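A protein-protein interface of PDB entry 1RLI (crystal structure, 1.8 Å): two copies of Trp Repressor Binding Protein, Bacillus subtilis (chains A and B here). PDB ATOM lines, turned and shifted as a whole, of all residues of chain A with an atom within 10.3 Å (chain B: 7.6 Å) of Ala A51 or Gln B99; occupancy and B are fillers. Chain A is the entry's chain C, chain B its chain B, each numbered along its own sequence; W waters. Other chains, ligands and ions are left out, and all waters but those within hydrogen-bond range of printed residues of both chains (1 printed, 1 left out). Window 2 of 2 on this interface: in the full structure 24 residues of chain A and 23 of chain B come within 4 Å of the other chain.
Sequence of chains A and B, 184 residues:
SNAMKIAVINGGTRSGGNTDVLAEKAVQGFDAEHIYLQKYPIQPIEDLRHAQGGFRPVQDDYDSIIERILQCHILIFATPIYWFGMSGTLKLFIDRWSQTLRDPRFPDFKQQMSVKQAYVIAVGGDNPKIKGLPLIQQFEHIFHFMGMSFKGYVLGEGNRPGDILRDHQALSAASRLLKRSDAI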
ATOM      1  N   THR A  13      10.641  17.055   1.057  1.00  0.00           N
ATOM      2  CA  THR A  13      11.098  15.697   1.326  1.00  0.00           C
ATOM      3  C   THR A  13      12.526  15.898   1.807  1.00  0.00           C
ATOM      4  O   THR A  13      13.298  16.634   1.193  1.00  0.00           O
ATOM      5  CB  THR A  13      11.083  14.815   0.058  1.00  0.00           C
ATOM      6  OG1 THR A  13       9.949  13.938   0.107  1.00  0.00           O
ATOM      7  CG2 THR A  13      12.371  13.984  -0.044  1.00  0.00           C
ATOM      8  N   LYS A  39       4.225  13.344   6.787  1.00  0.00           N
ATOM      9  CA  LYS A  39       3.345  12.857   5.733  1.00  0.00           C
ATOM     10  C   LYS A  39       3.655  11.391   5.478  1.00  0.00           C
ATOM     11  O   LYS A  39       4.808  10.957   5.549  1.00  0.00           O
ATOM     12  CB  LYS A  39       3.500  13.665   4.438  1.00  0.00           C
ATOM     13  CG  LYS A  39       4.864  13.608   3.772  1.00  0.00           C
ATOM     14  CD  LYS A  39       4.827  14.357   2.444  1.00  0.00           C
ATOM     15  CE  LYS A  39       6.210  14.550   1.843  1.00  0.00           C
ATOM     16  NZ  LYS A  39       6.147  15.110   0.465  1.00  0.00           N
ATOM     17  N   TYR A  40       2.615  10.619   5.198  1.00  0.00           N
ATOM     18  CA  TYR A  40       2.788   9.201   4.951  1.00  0.00           C
ATOM     19  C   TYR A  40       2.074   8.809   3.677  1.00  0.00           C
ATOM     20  O   TYR A  40       1.139   9.485   3.247  1.00  0.00           O
ATOM     21  CB  TYR A  40       2.258   8.399   6.143  1.00  0.00           C
ATOM     22  CG  TYR A  40       3.139   8.546   7.360  1.00  0.00           C
ATOM     23  CD1 TYR A  40       4.371   7.893   7.433  1.00  0.00           C
ATOM     24  CD2 TYR A  40       2.782   9.399   8.405  1.00  0.00           C
ATOM     25  CE1 TYR A  40       5.231   8.090   8.513  1.00  0.00           C
ATOM     26  CE2 TYR A  40       3.637   9.606   9.490  1.00  0.00           C
ATOM     27  CZ  TYR A  40       4.859   8.947   9.536  1.00  0.00           C
ATOM     28  OH  TYR A  40       5.706   9.140  10.605  1.00  0.00           O
ATOM     29  N   PRO A  41       2.524   7.722   3.044  1.00  0.00           N
ATOM     30  CA  PRO A  41       1.926   7.230   1.800  1.00  0.00           C
ATOM     31  C   PRO A  41       0.470   6.798   1.975  1.00  0.00           C
ATOM     32  O   PRO A  41      -0.389   7.128   1.152  1.00  0.00           O
ATOM     33  CB  PRO A  41       2.845   6.071   1.417  1.00  0.00           C
ATOM     34  CG  PRO A  41       3.349   5.581   2.747  1.00  0.00           C
ATOM     35  CD  PRO A  41       3.649   6.867   3.463  1.00  0.00           C
ATOM     36  N   ALA A  51       6.588  10.067  -6.474  1.00  0.00           N
ATOM     37  CA  ALA A  51       5.857   9.950  -5.216  1.00  0.00           C
ATOM     38  C   ALA A  51       4.996  11.176  -4.898  1.00  0.00           C
ATOM     39  O   ALA A  51       4.085  11.096  -4.077  1.00  0.00           O
ATOM     40  CB  ALA A  51       6.835   9.696  -4.064  1.00  0.00           C
ATOM     41  N   GLN A  52       5.286  12.305  -5.537  1.00  0.00           N
ATOM     42  CA  GLN A  52       4.527  13.532  -5.287  1.00  0.00           C
ATOM     43  C   GLN A  52       3.019  13.293  -5.422  1.00  0.00           C
ATOM     44  O   GLN A  52       2.551  12.757  -6.428  1.00  0.00           O
ATOM     45  CB  GLN A  52       4.965  14.640  -6.253  1.00  0.00           C
ATOM     46  CG  GLN A  52       6.473  14.730  -6.462  1.00  0.00           C
ATOM     47  CD  GLN A  52       6.938  16.122  -6.873  1.00  0.00           C
ATOM     48  OE1 GLN A  52       6.323  16.779  -7.719  1.00  0.00           O
ATOM     49  NE2 GLN A  52       8.042  16.572  -6.279  1.00  0.00           N
ATOM     50  N   GLY A  53       2.269  13.689  -4.396  1.00  0.00           N
ATOM     51  CA  GLY A  53       0.827  13.503  -4.412  1.00  0.00           C
ATOM     52  C   GLY A  53       0.409  12.140  -3.881  1.00  0.00           C
ATOM     53  O   GLY A  53      -0.782  11.816  -3.840  1.00  0.00           O
ATOM     54  N   GLY A  54       1.390  11.346  -3.459  1.00  0.00           N
ATOM     55  CA  GLY A  54       1.104  10.020  -2.941  1.00  0.00           C
ATOM     56  C   GLY A  54       1.060   9.928  -1.429  1.00  0.00           C
ATOM     57  O   GLY A  54       0.962   8.827  -0.874  1.00  0.00           O
ATOM     58  N   PHE A  55       1.144  11.074  -0.758  1.00  0.00           N
ATOM     59  CA  PHE A  55       1.100  11.103   0.698  1.00  0.00           C
ATOM     60  C   PHE A  55      -0.094  11.891   1.205  1.00  0.00           C
ATOM     61  O   PHE A  55      -0.835  12.506   0.438  1.00  0.00           O
ATOM     62  CB  PHE A  55       2.357  11.755   1.292  1.00  0.00           C
ATOM     63  CG  PHE A  55       3.642  11.126   0.859  1.00  0.00           C
ATOM     64  CD1 PHE A  55       4.255  11.512  -0.334  1.00  0.00           C
ATOM     65  CD2 PHE A  55       4.262  10.166   1.654  1.00  0.00           C
ATOM     66  CE1 PHE A  55       5.468  10.954  -0.725  1.00  0.00           C
ATOM     67  CE2 PHE A  55       5.476   9.599   1.268  1.00  0.00           C
ATOM     68  CZ  PHE A  55       6.080   9.996   0.078  1.00  0.00           C
ATOM     69  N   ARG A  56      -0.249  11.869   2.521  1.00  0.00           N
ATOM     70  CA  ARG A  56      -1.299  12.597   3.218  1.00  0.00           C
ATOM     71  C   ARG A  56      -0.597  13.155   4.447  1.00  0.00           C
ATOM     72  O   ARG A  56       0.012  12.408   5.218  1.00  0.00           O
ATOM     73  CB  ARG A  56      -2.430  11.661   3.657  1.00  0.00           C
ATOM     74  CG  ARG A  56      -3.532  12.362   4.444  1.00  0.00           C
ATOM     75  CD  ARG A  56      -4.634  11.391   4.878  1.00  0.00           C
ATOM     76  NE  ARG A  56      -5.695  12.057   5.634  1.00  0.00           N
ATOM     77  CZ  ARG A  56      -6.794  11.455   6.082  1.00  0.00           C
ATOM     78  NH1 ARG A  56      -6.989  10.161   5.854  1.00  0.00           N
ATOM     79  NH2 ARG A  56      -7.706  12.150   6.755  1.00  0.00           N
ATOM     80  N   TYR A  82       4.805  22.764  -5.819  1.00  0.00           N
ATOM     81  CA  TYR A  82       3.945  21.725  -6.410  1.00  0.00           C
ATOM     82  C   TYR A  82       2.747  22.402  -7.040  1.00  0.00           C
ATOM     83  O   TYR A  82       1.991  23.080  -6.345  1.00  0.00           O
ATOM     84  CB  TYR A  82       3.388  20.758  -5.358  1.00  0.00           C
ATOM     85  CG  TYR A  82       4.384  19.853  -4.674  1.00  0.00           C
ATOM     86  CD1 TYR A  82       5.591  19.514  -5.279  1.00  0.00           C
ATOM     87  CD2 TYR A  82       4.092  19.305  -3.427  1.00  0.00           C
ATOM     88  CE1 TYR A  82       6.489  18.640  -4.647  1.00  0.00           C
ATOM     89  CE2 TYR A  82       4.975  18.440  -2.794  1.00  0.00           C
ATOM     90  CZ  TYR A  82       6.168  18.114  -3.407  1.00  0.00           C
ATOM     91  OH  TYR A  82       7.045  17.264  -2.763  1.00  0.00           O
ATOM     92  N   TRP A  83       2.553  22.194  -8.340  1.00  0.00           N
ATOM     93  CA  TRP A  83       1.417  22.790  -9.037  1.00  0.00           C
ATOM     94  C   TRP A  83       1.327  24.303  -8.787  1.00  0.00           C
ATOM     95  O   TRP A  83       0.258  24.851  -8.486  1.00  0.00           O
ATOM     96  CB  TRP A  83       0.135  22.072  -8.619  1.00  0.00           C
ATOM     97  CG  TRP A  83       0.132  20.657  -9.097  1.00  0.00           C
ATOM     98  CD1 TRP A  83       0.576  19.550  -8.423  1.00  0.00           C
ATOM     99  CD2 TRP A  83      -0.224  20.218 -10.408  1.00  0.00           C
ATOM    100  NE1 TRP A  83       0.520  18.445  -9.248  1.00  0.00           N
ATOM    101  CE2 TRP A  83       0.032  18.828 -10.471  1.00  0.00           C
ATOM    102  CE3 TRP A  83      -0.735  20.868 -11.542  1.00  0.00           C
ATOM    103  CZ2 TRP A  83      -0.204  18.074 -11.625  1.00  0.00           C
ATOM    104  CZ3 TRP A  83      -0.975  20.125 -12.695  1.00  0.00           C
ATOM    105  CH2 TRP A  83      -0.706  18.735 -12.726  1.00  0.00           C
ATOM    106  N   GLY A  88       1.659  20.212  -0.066  1.00  0.00           N
ATOM    107  CA  GLY A  88       0.411  19.910   0.626  1.00  0.00           C
ATOM    108  C   GLY A  88       0.593  20.011   2.136  1.00  0.00           C
ATOM    109  O   GLY A  88      -0.287  20.510   2.857  1.00  0.00           O
ATOM    110  N   ASN A 159      14.317  19.747 -10.161  1.00  0.00           N
ATOM    111  CA  ASN A 159      13.220  18.789 -10.255  1.00  0.00           C
ATOM    112  C   ASN A 159      13.616  17.423  -9.697  1.00  0.00           C
ATOM    113  O   ASN A 159      12.753  16.621  -9.336  1.00  0.00           O
ATOM    114  CB  ASN A 159      12.769  18.635 -11.709  1.00  0.00           C
ATOM    115  CG  ASN A 159      13.842  18.029 -12.589  1.00  0.00           C
ATOM    116  OD1 ASN A 159      14.927  18.593 -12.740  1.00  0.00           O
ATOM    117  ND2 ASN A 159      13.545  16.872 -13.176  1.00  0.00           N
ATOM    118  N   ARG A 160      14.920  17.166  -9.638  1.00  0.00           N
ATOM    119  CA  ARG A 160      15.452  15.906  -9.117  1.00  0.00           C
ATOM    120  C   ARG A 160      16.491  16.172  -8.027  1.00  0.00           C
ATOM    121  O   ARG A 160      17.224  17.159  -8.080  1.00  0.00           O
ATOM    122  CB  ARG A 160      16.101  15.091 -10.241  1.00  0.00           C
ATOM    123  CG  ARG A 160      15.127  14.551 -11.277  1.00  0.00           C
ATOM    124  CD  ARG A 160      14.148  13.562 -10.659  1.00  0.00           C
ATOM    125  NE  ARG A 160      13.281  12.946 -11.661  1.00  0.00           N
ATOM    126  CZ  ARG A 160      12.351  12.034 -11.391  1.00  0.00           C
ATOM    127  NH1 ARG A 160      12.160  11.626 -10.140  1.00  0.00           N
ATOM    128  NH2 ARG A 160      11.617  11.521 -12.371  1.00  0.00           N
ATOM    129  N   PRO A 161      16.561  15.290  -7.018  1.00  0.00           N
ATOM    130  CA  PRO A 161      17.521  15.451  -5.923  1.00  0.00           C
ATOM    131  C   PRO A 161      18.927  15.749  -6.433  1.00  0.00           C
ATOM    132  O   PRO A 161      19.426  15.074  -7.337  1.00  0.00           O
ATOM    133  CB  PRO A 161      17.440  14.110  -5.204  1.00  0.00           C
ATOM    134  CG  PRO A 161      16.011  13.740  -5.374  1.00  0.00           C
ATOM    135  CD  PRO A 161      15.754  14.072  -6.829  1.00  0.00           C
ATOM    136  N   TYR B  62     -11.399   9.280  -4.675  1.00  0.00           N
ATOM    137  CA  TYR B  62     -10.621  10.072  -5.625  1.00  0.00           C
ATOM    138  C   TYR B  62     -10.761   9.555  -7.056  1.00  0.00           C
ATOM    139  O   TYR B  62     -11.017  10.320  -7.985  1.00  0.00           O
ATOM    140  CB  TYR B  62      -9.138  10.060  -5.241  1.00  0.00           C
ATOM    141  CG  TYR B  62      -8.249  10.801  -6.222  1.00  0.00           C
ATOM    142  CD1 TYR B  62      -8.135  12.189  -6.182  1.00  0.00           C
ATOM    143  CD2 TYR B  62      -7.543  10.109  -7.206  1.00  0.00           C
ATOM    144  CE1 TYR B  62      -7.336  12.871  -7.095  1.00  0.00           C
ATOM    145  CE2 TYR B  62      -6.742  10.779  -8.127  1.00  0.00           C
ATOM    146  CZ  TYR B  62      -6.641  12.168  -8.061  1.00  0.00           C
ATOM    147  OH  TYR B  62      -5.835  12.840  -8.951  1.00  0.00           O
ATOM    148  N   ILE B  94      -5.772  18.550  -6.441  1.00  0.00           N
ATOM    149  CA  ILE B  94      -4.940  18.862  -7.605  1.00  0.00           C
ATOM    150  C   ILE B  94      -3.538  18.247  -7.463  1.00  0.00           C
ATOM    151  O   ILE B  94      -2.968  17.759  -8.435  1.00  0.00           O
ATOM    152  CB  ILE B  94      -4.830  20.401  -7.833  1.00  0.00           C
ATOM    153  CG1 ILE B  94      -6.213  20.948  -8.223  1.00  0.00           C
ATOM    154  CG2 ILE B  94      -3.808  20.691  -8.953  1.00  0.00           C
ATOM    155  CD1 ILE B  94      -6.341  22.483  -8.151  1.00  0.00           C
ATOM    156  N   ASP B  95      -2.978  18.261  -6.261  1.00  0.00           N
ATOM    157  CA  ASP B  95      -1.657  17.681  -6.084  1.00  0.00           C
ATOM    158  C   ASP B  95      -1.640  16.217  -6.528  1.00  0.00           C
ATOM    159  O   ASP B  95      -0.659  15.752  -7.120  1.00  0.00           O
ATOM    160  CB  ASP B  95      -1.219  17.774  -4.621  1.00  0.00           C
ATOM    161  CG  ASP B  95      -0.545  19.089  -4.297  1.00  0.00           C
ATOM    162  OD1 ASP B  95      -0.400  19.923  -5.221  1.00  0.00           O
ATOM    163  OD2 ASP B  95      -0.161  19.286  -3.111  1.00  0.00           O
ATOM    164  N   ARG B  96      -2.729  15.495  -6.278  1.00  0.00           N
ATOM    165  CA  ARG B  96      -2.747  14.095  -6.657  1.00  0.00           C
ATOM    166  C   ARG B  96      -2.788  13.862  -8.160  1.00  0.00           C
ATOM    167  O   ARG B  96      -2.623  12.723  -8.623  1.00  0.00           O
ATOM    168  CB  ARG B  96      -3.889  13.339  -5.966  1.00  0.00           C
ATOM    169  CG  ARG B  96      -3.454  11.911  -5.687  1.00  0.00           C
ATOM    170  CD  ARG B  96      -4.560  10.900  -5.665  1.00  0.00           C
ATOM    171  NE  ARG B  96      -5.212  10.798  -4.371  1.00  0.00           N
ATOM    172  CZ  ARG B  96      -5.817   9.696  -3.942  1.00  0.00           C
ATOM    173  NH1 ARG B  96      -5.841   8.611  -4.703  1.00  0.00           N
ATOM    174  NH2 ARG B  96      -6.409   9.680  -2.758  1.00  0.00           N
ATOM    175  N   TRP B  97      -2.982  14.928  -8.936  1.00  0.00           N
ATOM    176  CA  TRP B  97      -2.981  14.777 -10.389  1.00  0.00           C
ATOM    177  C   TRP B  97      -1.618  14.287 -10.844  1.00  0.00           C
ATOM    178  O   TRP B  97      -1.491  13.734 -11.941  1.00  0.00           O
ATOM    179  CB  TRP B  97      -3.267  16.096 -11.113  1.00  0.00           C
ATOM    180  CG  TRP B  97      -4.675  16.589 -10.983  1.00  0.00           C
ATOM    181  CD1 TRP B  97      -5.698  15.971 -10.351  1.00  0.00           C
ATOM    182  CD2 TRP B  97      -5.211  17.799 -11.540  1.00  0.00           C
ATOM    183  NE1 TRP B  97      -6.854  16.712 -10.472  1.00  0.00           N
ATOM    184  CE2 TRP B  97      -6.582  17.840 -11.201  1.00  0.00           C
ATOM    185  CE3 TRP B  97      -4.667  18.849 -12.293  1.00  0.00           C
ATOM    186  CZ2 TRP B  97      -7.428  18.897 -11.586  1.00  0.00           C
ATOM    187  CZ3 TRP B  97      -5.511  19.905 -12.678  1.00  0.00           C
ATOM    188  CH2 TRP B  97      -6.872  19.914 -12.318  1.00  0.00           C
ATOM    189  N   SER B  98      -0.598  14.516 -10.019  1.00  0.00           N
ATOM    190  CA  SER B  98       0.747  14.079 -10.345  1.00  0.00           C
ATOM    191  C   SER B  98       0.764  12.548 -10.406  1.00  0.00           C
ATOM    192  O   SER B  98       1.510  11.964 -11.201  1.00  0.00           O
ATOM    193  CB  SER B  98       1.744  14.577  -9.290  1.00  0.00           C
ATOM    194  OG  SER B  98       2.049  15.950  -9.494  1.00  0.00           O
ATOM    195  N   GLN B  99      -0.043  11.914  -9.564  1.00  0.00           N
ATOM    196  CA  GLN B  99      -0.124  10.449  -9.531  1.00  0.00           C
ATOM    197  C   GLN B  99      -0.929   9.974 -10.724  1.00  0.00           C
ATOM    198  O   GLN B  99      -0.575   8.987 -11.379  1.00  0.00           O
ATOM    199  CB  GLN B  99      -0.800   9.953  -8.241  1.00  0.00           C
ATOM    200  CG  GLN B  99       0.037  10.111  -6.978  1.00  0.00           C
ATOM    201  CD  GLN B  99       1.320   9.286  -7.019  1.00  0.00           C
ATOM    202  OE1 GLN B  99       1.280   8.053  -7.102  1.00  0.00           O
ATOM    203  NE2 GLN B  99       2.461   9.966  -6.967  1.00  0.00           N
ATOM    204  N   THR B 100      -2.010  10.692 -11.016  1.00  0.00           N
ATOM    205  CA  THR B 100      -2.881  10.337 -12.134  1.00  0.00           C
ATOM    206  C   THR B 100      -2.181  10.508 -13.481  1.00  0.00           C
ATOM    207  O   THR B 100      -2.466   9.786 -14.434  1.00  0.00           O
ATOM    208  CB  THR B 100      -4.198  11.168 -12.081  1.00  0.00           C
ATOM    209  OG1 THR B 100      -4.815  10.969 -10.800  1.00  0.00           O
ATOM    210  CG2 THR B 100      -5.185  10.698 -13.138  1.00  0.00           C
ATOM    211  N   LEU B 101      -1.254  11.453 -13.569  1.00  0.00           N
ATOM    212  CA  LEU B 101      -0.523  11.649 -14.812  1.00  0.00           C
ATOM    213  C   LEU B 101       0.337  10.428 -15.159  1.00  0.00           C
ATOM    214  O   LEU B 101       0.841  10.317 -16.272  1.00  0.00           O
ATOM    215  CB  LEU B 101       0.361  12.895 -14.717  1.00  0.00           C
ATOM    216  CG  LEU B 101      -0.404  14.213 -14.858  1.00  0.00           C
ATOM    217  CD1 LEU B 101       0.436  15.359 -14.318  1.00  0.00           C
ATOM    218  CD2 LEU B 101      -0.757  14.432 -16.334  1.00  0.00           C
ATOM    219  N   ARG B 102       0.488   9.516 -14.207  1.00  0.00           N
ATOM    220  CA  ARG B 102       1.289   8.313 -14.426  1.00  0.00           C
ATOM    221  C   ARG B 102       0.507   7.029 -14.112  1.00  0.00           C
ATOM    222  O   ARG B 102       1.088   5.946 -14.040  1.00  0.00           O
ATOM    223  CB  ARG B 102       2.547   8.383 -13.555  1.00  0.00           C
ATOM    224  CG  ARG B 102       3.434   9.588 -13.856  1.00  0.00           C
ATOM    225  CD  ARG B 102       4.487   9.784 -12.773  1.00  0.00           C
ATOM    226  NE  ARG B 102       5.396   8.648 -12.695  1.00  0.00           N
ATOM    227  CZ  ARG B 102       6.270   8.330 -13.642  1.00  0.00           C
ATOM    228  NH1 ARG B 102       6.354   9.068 -14.742  1.00  0.00           N
ATOM    229  NH2 ARG B 102       7.051   7.268 -13.495  1.00  0.00           N
ATOM    230  N   ASP B 103      -0.809   7.158 -13.930  1.00  0.00           N
ATOM    231  CA  ASP B 103      -1.686   6.024 -13.604  1.00  0.00           C
ATOM    232  C   ASP B 103      -2.094   5.302 -14.895  1.00  0.00           C
ATOM    233  O   ASP B 103      -2.729   5.885 -15.771  1.00  0.00           O
ATOM    234  CB  ASP B 103      -2.930   6.550 -12.870  1.00  0.00           C
ATOM    235  CG  ASP B 103      -3.735   5.455 -12.190  1.00  0.00           C
ATOM    236  OD1 ASP B 103      -3.828   4.324 -12.731  1.00  0.00           O
ATOM    237  OD2 ASP B 103      -4.309   5.736 -11.111  1.00  0.00           O
ATOM    238  N   PRO B 104      -1.736   4.011 -15.029  1.00  0.00           N
ATOM    239  CA  PRO B 104      -2.107   3.298 -16.256  1.00  0.00           C
ATOM    240  C   PRO B 104      -3.610   3.099 -16.475  1.00  0.00           C
ATOM    241  O   PRO B 104      -4.038   2.762 -17.582  1.00  0.00           O
ATOM    242  CB  PRO B 104      -1.332   1.982 -16.142  1.00  0.00           C
ATOM    243  CG  PRO B 104      -1.264   1.758 -14.663  1.00  0.00           C
ATOM    244  CD  PRO B 104      -0.972   3.143 -14.116  1.00  0.00           C
ATOM    245  N   ARG B 105      -4.406   3.309 -15.430  1.00  0.00           N
ATOM    246  CA  ARG B 105      -5.856   3.172 -15.539  1.00  0.00           C
ATOM    247  C   ARG B 105      -6.465   4.404 -16.218  1.00  0.00           C
ATOM    248  O   ARG B 105      -7.579   4.348 -16.742  1.00  0.00           O
ATOM    249  CB  ARG B 105      -6.475   2.995 -14.155  1.00  0.00           C
ATOM    250  CG  ARG B 105      -6.008   1.757 -13.418  1.00  0.00           C
ATOM    251  CD  ARG B 105      -6.543   1.770 -12.004  1.00  0.00           C
ATOM    252  NE  ARG B 105      -6.068   2.942 -11.272  1.00  0.00           N
ATOM    253  CZ  ARG B 105      -6.572   3.334 -10.111  1.00  0.00           C
ATOM    254  NH1 ARG B 105      -7.562   2.643  -9.561  1.00  0.00           N
ATOM    255  NH2 ARG B 105      -6.098   4.421  -9.507  1.00  0.00           N
ATOM    256  N   PHE B 106      -5.729   5.512 -16.199  1.00  0.00           N
ATOM    257  CA  PHE B 106      -6.165   6.771 -16.825  1.00  0.00           C
ATOM    258  C   PHE B 106      -5.073   7.253 -17.776  1.00  0.00           C
ATOM    259  O   PHE B 106      -4.541   8.362 -17.619  1.00  0.00           O
ATOM    260  CB  PHE B 106      -6.376   7.846 -15.751  1.00  0.00           C
ATOM    261  CG  PHE B 106      -7.456   7.517 -14.761  1.00  0.00           C
ATOM    262  CD1 PHE B 106      -8.792   7.752 -15.068  1.00  0.00           C
ATOM    263  CD2 PHE B 106      -7.137   6.992 -13.512  1.00  0.00           C
ATOM    264  CE1 PHE B 106      -9.797   7.472 -14.141  1.00  0.00           C
ATOM    265  CE2 PHE B 106      -8.132   6.708 -12.582  1.00  0.00           C
ATOM    266  CZ  PHE B 106      -9.459   6.948 -12.896  1.00  0.00           C
ATOM    267  N   PHE B 109      -5.471  10.836 -19.351  1.00  0.00           N
ATOM    268  CA  PHE B 109      -5.841  11.917 -18.449  1.00  0.00           C
ATOM    269  C   PHE B 109      -5.430  13.311 -18.927  1.00  0.00           C
ATOM    270  O   PHE B 109      -6.263  14.214 -19.025  1.00  0.00           O
ATOM    271  CB  PHE B 109      -5.244  11.672 -17.067  1.00  0.00           C
ATOM    272  CG  PHE B 109      -5.557  12.753 -16.076  1.00  0.00           C
ATOM    273  CD1 PHE B 109      -6.868  12.985 -15.668  1.00  0.00           C
ATOM    274  CD2 PHE B 109      -4.540  13.535 -15.545  1.00  0.00           C
ATOM    275  CE1 PHE B 109      -7.165  13.982 -14.737  1.00  0.00           C
ATOM    276  CE2 PHE B 109      -4.827  14.533 -14.614  1.00  0.00           C
ATOM    277  CZ  PHE B 109      -6.139  14.755 -14.210  1.00  0.00           C
HETATM  278  O   HOH W   1       1.977  16.738  -3.402  1.00  0.00           O
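Ala A51 touches Gln B99.
Ser B98 touches Gln A52.
CG of Arg B96 touches O of Gly A53, at 3.2 Å.
Gln B99 touches Gly A54.
CB of Tyr A82 touches OD1 of Asp B95 (3.9 Å).
Ile B94 touches Trp A83 (O to NE1, 3.6 Å).
Trp A83 touches Asp B95.
Trp A83 touches Trp B97.
Trp A83 touches Leu B101.
OD2 of Asp B95 touches N of Gly A88, 3.7 Å away.
The backbone carbonyl oxygen (O) of Gln A52 sits at hydrogen-bond distance from the side-chain amide nitrogen (NE2) of Gln B99, at 2.8 Å.
OG of Ser B98 is in hydrogen-bond range of NE1 of Trp A83.
Of chain B, only Gln B99 comes within 4 Å of Ala A51.
Of the printed residues of chain B, Gln A52 touches Ser B98 (3.5 Å) and Gln B99 (2.8 Å).
Phe A55 touches none of the printed residues of chain B.
Printed residues of chain B within 4 Å of Gly A88: Asp B95.
No residue of chain A comes within 4 Å of Thr B100.
The nearest residue of chain B that does not touch Ala A51 is Ser B98 (6.4 Å).
The nearest residue of chain A that does not touch Gln B99 is Phe A55 (6.4 Å).
Water W1 lies within hydrogen-bond range of N of Gly A53 (3.2 Å) and OD2 of Asp B95 (3.3 Å).
No position is printed for both chains.
Of the 14 pairs that touch across the chains among the printed residues, none has its exchanged pair printed and touching as well.
OH of Tyr B62 is in hydrogen-bond range of O of Arg B96, 3.2 Å away.
Printed residues of chain B that touch a printed residue of chain A: Ile B94, Asp B95, Arg B96, Trp B97, Ser B98, Gln B99 and Leu B101.
Hydrophobic or aromatic side chains of chain B that line the printed part of chain A: Ile B94, Trp B97 and Leu B101.
Printed residues of chain A that touch a printed residue of chain B: Ala A51, Gln A52, Gly A53, Gly A54, Tyr A82, Trp A83 and Gly A88.
Hydrophobic or aromatic side chains of chain A that line the printed part of chain B: Tyr A82 and Trp A83.
Among the printed residues, 14 pairs touch across the chains.
Among the printed residues, no Asp or Glu carboxylate lies within 4 Å of a Lys or Arg side-chain nitrogen of the other chain.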
